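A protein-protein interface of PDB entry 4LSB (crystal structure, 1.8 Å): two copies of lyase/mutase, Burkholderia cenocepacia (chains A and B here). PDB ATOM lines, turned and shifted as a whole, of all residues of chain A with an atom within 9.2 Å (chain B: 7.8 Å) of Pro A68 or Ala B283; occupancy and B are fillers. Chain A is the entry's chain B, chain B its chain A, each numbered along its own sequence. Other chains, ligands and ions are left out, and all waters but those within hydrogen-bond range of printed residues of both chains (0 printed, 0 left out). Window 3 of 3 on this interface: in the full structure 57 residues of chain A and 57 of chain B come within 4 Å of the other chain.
NH2 of Arg B44 sits at hydrogen-bond distance from O of Asp B286 (3.0 Å).
O of Gly B275 sits at hydrogen-bond distance from ND2 of Asn B279.
The backbone carbonyl oxygen of Ala A62 lies within hydrogen-bond range of the backbone NH of Gln A67 (3.0 Å).
The backbone carbonyl oxygen of Phe B282 lies within hydrogen-bond range of the guanidinium group of Arg B44 (2.9 Å).
The side-chain hydroxyl (OG) of Ser A58 lies close to the side-chain carboxylate (OD1) of Asp A69, at 3.4 Å.
O of Ala B284 lies within hydrogen-bond range of NH2 of Arg B44.
The side-chain amide oxygen of Asn B279 is in hydrogen-bond range of the backbone NH of Asp A69, at 2.8 Å.
The backbone carbonyl oxygen (O) of Gly A66 sits at hydrogen-bond distance from the guanidinium group (NH1) of Arg B44 (2.8 Å).
Among the printed residues, merely in contact across the chains: Pro A68 with Ala B283 (3.4 Å), Phe A63 with Phe B282 (3.4 Å), Pro A68 with Asn B279 (3.4 Å), Phe A63 with Ile B278 (3.5 Å), Gly A66 with Phe B282 (3.6 Å), Phe A63 with Asn B279 (3.6 Å), Gln A67 with Phe B282 (3.6 Å) and Pro A68 with Phe B282 (3.6 Å).
Of the 15 printed residues of chain A, 5 touch a printed residue of chain B.
Printed residues of chain A that touch a printed residue of chain B: Phe A63, Gly A66, Gln A67, Pro A68 and Asp A69.
Of the 13 printed residues of chain B, 5 touch a printed residue of chain A.
Printed residues of chain B that touch a printed residue of chain A: Arg B44, Ile B278, Asn B279, Phe B282 and Ala B283.
Hydrophobic or aromatic side chains of chain B that line the printed part of chain A: Ile B278, Phe B282 and Ala B283.
No position is printed for both chains.
Of the 10 pairs that touch across the chains among the printed residues, none has its exchanged pair printed and touching as well.
Printed residues of chain B within 4 Å of Phe A63: Ile B278, Asn B279 and Phe B282.
Printed residues of chain B within 4 Å of Gln A67: Phe B282 (3.6 Å).
Pro A68 touches just these residues of chain B: Asn B279, Phe B282 and Ala B283.
Printed residues of chain B within 4 Å of Asp A69: Asn B279.
Printed residues of chain A within 4 Å of Ile B278: Phe A63 (3.5 Å).
Of the printed residues of chain A, Phe B282 touches Phe A63, Gly A66, Gln A67 and Pro A68.
Of chain A, only Pro A68 (3.4 Å) comes within 4 Å of Ala B283.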
ATOM      1  N   SER A  58       1.711 -11.015 -12.335  1.00  0.00           N
ATOM      2  CA  SER A  58       2.857 -10.141 -12.119  1.00  0.00           C
ATOM      3  C   SER A  58       3.434 -10.352 -10.690  1.00  0.00           C
ATOM      4  O   SER A  58       4.643 -10.260 -10.484  1.00  0.00           O
ATOM      5  CB  SER A  58       2.440  -8.659 -12.329  1.00  0.00           C
ATOM      6  OG  SER A  58       1.428  -8.308 -11.368  1.00  0.00           O
ATOM      7  N   ALA A  59       2.594 -10.671  -9.716  1.00  0.00           N
ATOM      8  CA  ALA A  59       3.054 -10.903  -8.349  1.00  0.00           C
ATOM      9  C   ALA A  59       3.827 -12.204  -8.178  1.00  0.00           C
ATOM     10  O   ALA A  59       4.897 -12.214  -7.534  1.00  0.00           O
ATOM     11  CB  ALA A  59       1.893 -10.936  -7.385  1.00  0.00           C
ATOM     12  N   GLY A  60       3.268 -13.293  -8.727  1.00  0.00           N
ATOM     13  CA  GLY A  60       3.928 -14.616  -8.674  1.00  0.00           C
ATOM     14  C   GLY A  60       5.255 -14.598  -9.388  1.00  0.00           C
ATOM     15  O   GLY A  60       6.286 -15.139  -8.916  1.00  0.00           O
ATOM     16  N   TYR A  61       5.263 -13.915 -10.531  1.00  0.00           N
ATOM     17  CA  TYR A  61       6.469 -13.776 -11.303  1.00  0.00           C
ATOM     18  C   TYR A  61       7.540 -13.054 -10.524  1.00  0.00           C
ATOM     19  O   TYR A  61       8.677 -13.501 -10.506  1.00  0.00           O
ATOM     20  CB  TYR A  61       6.200 -13.048 -12.637  1.00  0.00           C
ATOM     21  CG  TYR A  61       7.450 -12.776 -13.472  1.00  0.00           C
ATOM     22  CD1 TYR A  61       7.937 -13.724 -14.336  1.00  0.00           C
ATOM     23  CD2 TYR A  61       8.140 -11.562 -13.373  1.00  0.00           C
ATOM     24  CE1 TYR A  61       9.072 -13.494 -15.101  1.00  0.00           C
ATOM     25  CE2 TYR A  61       9.293 -11.326 -14.117  1.00  0.00           C
ATOM     26  CZ  TYR A  61       9.744 -12.297 -14.989  1.00  0.00           C
ATOM     27  OH  TYR A  61      10.879 -12.072 -15.767  1.00  0.00           O
ATOM     28  N   ALA A  62       7.163 -11.941  -9.901  1.00  0.00           N
ATOM     29  CA  ALA A  62       8.064 -11.154  -9.099  1.00  0.00           C
ATOM     30  C   ALA A  62       8.621 -11.970  -7.962  1.00  0.00           C
ATOM     31  O   ALA A  62       9.825 -11.956  -7.788  1.00  0.00           O
ATOM     32  CB  ALA A  62       7.373  -9.910  -8.577  1.00  0.00           C
ATOM     33  N   PHE A  63       7.773 -12.663  -7.190  1.00  0.00           N
ATOM     34  CA  PHE A  63       8.252 -13.477  -6.079  1.00  0.00           C
ATOM     35  C   PHE A  63       9.294 -14.502  -6.536  1.00  0.00           C
ATOM     36  O   PHE A  63      10.307 -14.700  -5.831  1.00  0.00           O
ATOM     37  CB  PHE A  63       7.110 -14.194  -5.325  1.00  0.00           C
ATOM     38  CG  PHE A  63       6.011 -13.271  -4.858  1.00  0.00           C
ATOM     39  CD1 PHE A  63       6.281 -11.934  -4.561  1.00  0.00           C
ATOM     40  CD2 PHE A  63       4.721 -13.738  -4.716  1.00  0.00           C
ATOM     41  CE1 PHE A  63       5.253 -11.104  -4.148  1.00  0.00           C
ATOM     42  CE2 PHE A  63       3.695 -12.914  -4.340  1.00  0.00           C
ATOM     43  CZ  PHE A  63       3.983 -11.577  -4.044  1.00  0.00           C
ATOM     44  N   SER A  64       9.109 -15.081  -7.715  1.00  0.00           N
ATOM     45  CA  SER A  64      10.100 -16.038  -8.237  1.00  0.00           C
ATOM     46  C   SER A  64      11.448 -15.379  -8.448  1.00  0.00           C
ATOM     47  O   SER A  64      12.492 -16.016  -8.314  1.00  0.00           O
ATOM     48  CB  SER A  64       9.625 -16.746  -9.524  1.00  0.00           C
ATOM     49  OG  SER A  64       9.767 -15.929 -10.693  1.00  0.00           O
ATOM     50  N   LYS A  65      11.432 -14.092  -8.806  1.00  0.00           N
ATOM     51  CA  LYS A  65      12.663 -13.352  -9.011  1.00  0.00           C
ATOM     52  C   LYS A  65      13.217 -12.703  -7.727  1.00  0.00           C
ATOM     53  O   LYS A  65      14.184 -11.977  -7.816  1.00  0.00           O
ATOM     54  CB  LYS A  65      12.439 -12.242 -10.039  1.00  0.00           C
ATOM     55  CG  LYS A  65      12.005 -12.721 -11.394  1.00  0.00           C
ATOM     56  CD  LYS A  65      13.068 -13.508 -12.110  1.00  0.00           C
ATOM     57  CE  LYS A  65      12.556 -14.059 -13.438  1.00  0.00           C
ATOM     58  NZ  LYS A  65      13.064 -15.452 -13.729  1.00  0.00           N
ATOM     59  N   GLY A  66      12.575 -12.936  -6.588  1.00  0.00           N
ATOM     60  CA  GLY A  66      13.014 -12.389  -5.316  1.00  0.00           C
ATOM     61  C   GLY A  66      12.680 -10.899  -5.181  1.00  0.00           C
ATOM     62  O   GLY A  66      13.371 -10.182  -4.461  1.00  0.00           O
ATOM     63  N   GLN A  67      11.629 -10.454  -5.860  1.00  0.00           N
ATOM     64  CA  GLN A  67      11.258  -9.031  -5.878  1.00  0.00           C
ATOM     65  C   GLN A  67       9.853  -8.843  -5.396  1.00  0.00           C
ATOM     66  O   GLN A  67       9.021  -9.764  -5.516  1.00  0.00           O
ATOM     67  CB  GLN A  67      11.338  -8.486  -7.298  1.00  0.00           C
ATOM     68  CG  GLN A  67      12.716  -8.475  -7.879  1.00  0.00           C
ATOM     69  CD  GLN A  67      12.639  -8.401  -9.404  1.00  0.00           C
ATOM     70  OE1 GLN A  67      11.576  -8.593  -9.985  1.00  0.00           O
ATOM     71  NE2 GLN A  67      13.737  -8.093 -10.034  1.00  0.00           N
ATOM     72  N   PRO A  68       9.558  -7.654  -4.849  1.00  0.00           N
ATOM     73  CA  PRO A  68       8.193  -7.446  -4.466  1.00  0.00           C
ATOM     74  C   PRO A  68       7.368  -7.170  -5.704  1.00  0.00           C
ATOM     75  O   PRO A  68       7.905  -6.885  -6.754  1.00  0.00           O
ATOM     76  CB  PRO A  68       8.260  -6.244  -3.474  1.00  0.00           C
ATOM     77  CG  PRO A  68       9.695  -5.757  -3.504  1.00  0.00           C
ATOM     78  CD  PRO A  68      10.357  -6.428  -4.704  1.00  0.00           C
ATOM     79  N   ASP A  69       6.062  -7.335  -5.593  1.00  0.00           N
ATOM     80  CA  ASP A  69       5.184  -7.130  -6.723  1.00  0.00           C
ATOM     81  C   ASP A  69       5.373  -5.693  -7.291  1.00  0.00           C
ATOM     82  O   ASP A  69       5.486  -4.741  -6.537  1.00  0.00           O
ATOM     83  CB  ASP A  69       3.747  -7.429  -6.276  1.00  0.00           C
ATOM     84  CG  ASP A  69       2.745  -7.385  -7.408  1.00  0.00           C
ATOM     85  OD1 ASP A  69       3.100  -7.366  -8.608  1.00  0.00           O
ATOM     86  OD2 ASP A  69       1.578  -7.354  -7.046  1.00  0.00           O
ATOM     87  N   ASN A  70       5.526  -5.608  -8.606  1.00  0.00           N
ATOM     88  CA  ASN A  70       5.607  -4.368  -9.414  1.00  0.00           C
ATOM     89  C   ASN A  70       7.029  -3.926  -9.714  1.00  0.00           C
ATOM     90  O   ASN A  70       7.212  -2.978 -10.480  1.00  0.00           O
ATOM     91  CB  ASN A  70       4.795  -3.223  -8.803  1.00  0.00           C
ATOM     92  N   ILE A  72       6.959  -4.242 -12.968  1.00  0.00           N
ATOM     93  CA  ILE A  72       7.652  -5.239 -13.822  1.00  0.00           C
ATOM     94  C   ILE A  72       8.012  -4.662 -15.180  1.00  0.00           C
ATOM     95  O   ILE A  72       7.259  -3.850 -15.719  1.00  0.00           O
ATOM     96  CB  ILE A  72       6.794  -6.501 -13.989  1.00  0.00           C
ATOM     97  N   GLU A  97      -0.394  -5.169 -16.316  1.00  0.00           N
ATOM     98  CA  GLU A  97      -0.292  -4.069 -15.344  1.00  0.00           C
ATOM     99  C   GLU A  97      -1.150  -2.900 -15.851  1.00  0.00           C
ATOM    100  O   GLU A  97      -2.290  -3.102 -16.279  1.00  0.00           O
ATOM    101  CB  GLU A  97       1.184  -3.639 -15.216  1.00  0.00           C
ATOM    102  CG  GLU A  97       2.164  -4.787 -15.012  1.00  0.00           C
ATOM    103  CD  GLU A  97       2.383  -5.078 -13.547  1.00  0.00           C
ATOM    104  OE1 GLU A  97       3.514  -4.858 -13.047  1.00  0.00           O
ATOM    105  OE2 GLU A  97       1.409  -5.503 -12.918  1.00  0.00           O
ATOM    106  N   ARG B  44      16.736 -16.141  -1.698  1.00  0.00           N
ATOM    107  CA  ARG B  44      16.665 -15.057  -0.696  1.00  0.00           C
ATOM    108  C   ARG B  44      16.055 -15.546   0.599  1.00  0.00           C
ATOM    109  O   ARG B  44      16.579 -15.266   1.666  1.00  0.00           O
ATOM    110  CB  ARG B  44      15.831 -13.870  -1.182  1.00  0.00           C
ATOM    111  CG  ARG B  44      16.359 -13.204  -2.412  1.00  0.00           C
ATOM    112  CD  ARG B  44      15.767 -11.805  -2.624  1.00  0.00           C
ATOM    113  NE  ARG B  44      16.094 -10.934  -1.535  1.00  0.00           N
ATOM    114  CZ  ARG B  44      15.568  -9.728  -1.330  1.00  0.00           C
ATOM    115  NH1 ARG B  44      14.691  -9.241  -2.184  1.00  0.00           N
ATOM    116  NH2 ARG B  44      15.934  -9.003  -0.264  1.00  0.00           N
ATOM    117  N   MET B  48      17.456 -15.536   4.359  1.00  0.00           N
ATOM    118  CA  MET B  48      16.716 -14.910   5.488  1.00  0.00           C
ATOM    119  C   MET B  48      16.415 -15.873   6.630  1.00  0.00           C
ATOM    120  O   MET B  48      16.294 -15.436   7.772  1.00  0.00           O
ATOM    121  CB  MET B  48      15.409 -14.263   5.025  1.00  0.00           C
ATOM    122  CG  MET B  48      15.634 -13.057   4.137  1.00  0.00           C
ATOM    123  SD  MET B  48      14.087 -12.596   3.301  1.00  0.00           S
ATOM    124  CE  MET B  48      14.614 -11.409   2.074  1.00  0.00           C
ATOM    125  N   GLY B 275       0.482 -11.960   1.315  1.00  0.00           N
ATOM    126  CA  GLY B 275       1.117 -11.108   0.347  1.00  0.00           C
ATOM    127  C   GLY B 275       1.855  -9.942   0.945  1.00  0.00           C
ATOM    128  O   GLY B 275       2.872  -9.501   0.399  1.00  0.00           O
ATOM    129  N   ASP B 277       3.440  -9.853   3.833  1.00  0.00           N
ATOM    130  CA  ASP B 277       4.709 -10.353   4.373  1.00  0.00           C
ATOM    131  C   ASP B 277       5.805 -10.513   3.306  1.00  0.00           C
ATOM    132  O   ASP B 277       6.926 -10.016   3.510  1.00  0.00           O
ATOM    133  CB  ASP B 277       4.482 -11.697   5.102  1.00  0.00           C
ATOM    134  CG  ASP B 277       3.711 -11.521   6.407  1.00  0.00           C
ATOM    135  OD1 ASP B 277       3.627 -10.371   6.869  1.00  0.00           O
ATOM    136  OD2 ASP B 277       3.214 -12.507   6.975  1.00  0.00           O
ATOM    137  N   ILE B 278       5.484 -11.247   2.215  1.00  0.00           N
ATOM    138  CA  ILE B 278       6.426 -11.541   1.086  1.00  0.00           C
ATOM    139  C   ILE B 278       6.835 -10.253   0.366  1.00  0.00           C
ATOM    140  O   ILE B 278       8.001 -10.068  -0.034  1.00  0.00           O
ATOM    141  CB  ILE B 278       5.842 -12.658   0.131  1.00  0.00           C
ATOM    142  CG1 ILE B 278       6.847 -13.127  -0.914  1.00  0.00           C
ATOM    143  CG2 ILE B 278       4.603 -12.196  -0.629  1.00  0.00           C
ATOM    144  CD1 ILE B 278       7.820 -14.103  -0.340  1.00  0.00           C
ATOM    145  N   ASN B 279       5.905  -9.302   0.230  1.00  0.00           N
ATOM    146  CA  ASN B 279       6.301  -8.013  -0.327  1.00  0.00           C
ATOM    147  C   ASN B 279       7.246  -7.226   0.569  1.00  0.00           C
ATOM    148  O   ASN B 279       8.186  -6.629   0.078  1.00  0.00           O
ATOM    149  CB  ASN B 279       5.064  -7.188  -0.701  1.00  0.00           C
ATOM    150  CG  ASN B 279       4.438  -7.709  -1.978  1.00  0.00           C
ATOM    151  OD1 ASN B 279       5.088  -7.722  -3.009  1.00  0.00           O
ATOM    152  ND2 ASN B 279       3.209  -8.202  -1.896  1.00  0.00           N
ATOM    153  N   ARG B 280       6.996  -7.245   1.872  1.00  0.00           N
ATOM    154  CA  ARG B 280       7.863  -6.534   2.842  1.00  0.00           C
ATOM    155  C   ARG B 280       9.267  -7.134   2.813  1.00  0.00           C
ATOM    156  O   ARG B 280      10.246  -6.447   2.596  1.00  0.00           O
ATOM    157  CB  ARG B 280       7.241  -6.583   4.249  1.00  0.00           C
ATOM    158  CG  ARG B 280       8.161  -6.101   5.388  1.00  0.00           C
ATOM    159  CD  ARG B 280       7.497  -6.061   6.768  1.00  0.00           C
ATOM    160  NE  ARG B 280       7.396  -7.379   7.407  1.00  0.00           N
ATOM    161  CZ  ARG B 280       6.291  -8.136   7.434  1.00  0.00           C
ATOM    162  NH1 ARG B 280       5.163  -7.728   6.841  1.00  0.00           N
ATOM    163  NH2 ARG B 280       6.319  -9.338   8.036  1.00  0.00           N
ATOM    164  N   TRP B 281       9.361  -8.452   2.965  1.00  0.00           N
ATOM    165  CA  TRP B 281      10.668  -9.149   2.919  1.00  0.00           C
ATOM    166  C   TRP B 281      11.454  -8.914   1.651  1.00  0.00           C
ATOM    167  O   TRP B 281      12.622  -8.591   1.700  1.00  0.00           O
ATOM    168  CB  TRP B 281      10.485 -10.643   3.126  1.00  0.00           C
ATOM    169  CG  TRP B 281       9.790 -10.997   4.345  1.00  0.00           C
ATOM    170  CD1 TRP B 281       9.782 -10.303   5.528  1.00  0.00           C
ATOM    171  CD2 TRP B 281       9.037 -12.191   4.573  1.00  0.00           C
ATOM    172  NE1 TRP B 281       9.021 -10.976   6.456  1.00  0.00           N
ATOM    173  CE2 TRP B 281       8.573 -12.148   5.904  1.00  0.00           C
ATOM    174  CE3 TRP B 281       8.714 -13.307   3.777  1.00  0.00           C
ATOM    175  CZ2 TRP B 281       7.761 -13.167   6.458  1.00  0.00           C
ATOM    176  CZ3 TRP B 281       7.908 -14.322   4.329  1.00  0.00           C
ATOM    177  CH2 TRP B 281       7.439 -14.241   5.651  1.00  0.00           C
ATOM    178  N   PHE B 282      10.822  -9.014   0.498  1.00  0.00           N
ATOM    179  CA  PHE B 282      11.542  -8.839  -0.753  1.00  0.00           C
ATOM    180  C   PHE B 282      11.863  -7.374  -1.094  1.00  0.00           C
ATOM    181  O   PHE B 282      12.819  -7.120  -1.830  1.00  0.00           O
ATOM    182  CB  PHE B 282      10.832  -9.525  -1.928  1.00  0.00           C
ATOM    183  CG  PHE B 282      10.936 -11.042  -1.913  1.00  0.00           C
ATOM    184  CD1 PHE B 282      11.792 -11.690  -1.056  1.00  0.00           C
ATOM    185  CD2 PHE B 282      10.193 -11.798  -2.806  1.00  0.00           C
ATOM    186  CE1 PHE B 282      11.927 -13.049  -1.074  1.00  0.00           C
ATOM    187  CE2 PHE B 282      10.298 -13.192  -2.819  1.00  0.00           C
ATOM    188  CZ  PHE B 282      11.171 -13.812  -1.959  1.00  0.00           C
ATOM    189  N   ALA B 283      11.097  -6.424  -0.534  1.00  0.00           N
ATOM    190  CA  ALA B 283      11.451  -4.986  -0.636  1.00  0.00           C
ATOM    191  C   ALA B 283      12.778  -4.664   0.013  1.00  0.00           C
ATOM    192  O   ALA B 283      13.446  -3.756  -0.447  1.00  0.00           O
ATOM    193  CB  ALA B 283      10.353  -4.086  -0.064  1.00  0.00           C
ATOM    194  N   ALA B 284      13.171  -5.430   1.036  1.00  0.00           N
ATOM    195  CA  ALA B 284      14.483  -5.281   1.686  1.00  0.00           C
ATOM    196  C   ALA B 284      15.677  -5.325   0.704  1.00  0.00           C
ATOM    197  O   ALA B 284      15.655  -6.064  -0.303  1.00  0.00           O
ATOM    198  CB  ALA B 284      14.661  -6.322   2.773  1.00  0.00           C
ATOM    199  N   PRO B 285      16.713  -4.494   0.974  1.00  0.00           N
ATOM    200  CA  PRO B 285      17.867  -4.414   0.104  1.00  0.00           C
ATOM    201  C   PRO B 285      18.838  -5.563   0.368  1.00  0.00           C
ATOM    202  O   PRO B 285      19.827  -5.663  -0.315  1.00  0.00           O
ATOM    203  CB  PRO B 285      18.500  -3.064   0.496  1.00  0.00           C
ATOM    204  CG  PRO B 285      18.203  -2.944   1.952  1.00  0.00           C
ATOM    205  CD  PRO B 285      16.827  -3.540   2.104  1.00  0.00           C
ATOM    206  N   ASP B 286      18.565  -6.409   1.357  1.00  0.00           N
ATOM    207  CA  ASP B 286      19.412  -7.569   1.613  1.00  0.00           C
ATOM    208  C   ASP B 286      18.605  -8.684   2.271  1.00  0.00           C
ATOM    209  O   ASP B 286      17.386  -8.582   2.364  1.00  0.00           O
ATOM    210  CB  ASP B 286      20.653  -7.199   2.427  1.00  0.00           C
ATOM    211  CG  ASP B 286      20.334  -6.735   3.820  1.00  0.00           C
ATOM    212  OD1 ASP B 286      19.225  -6.970   4.346  1.00  0.00           O
ATOM    213  OD2 ASP B 286      21.232  -6.115   4.407  1.00  0.00           O
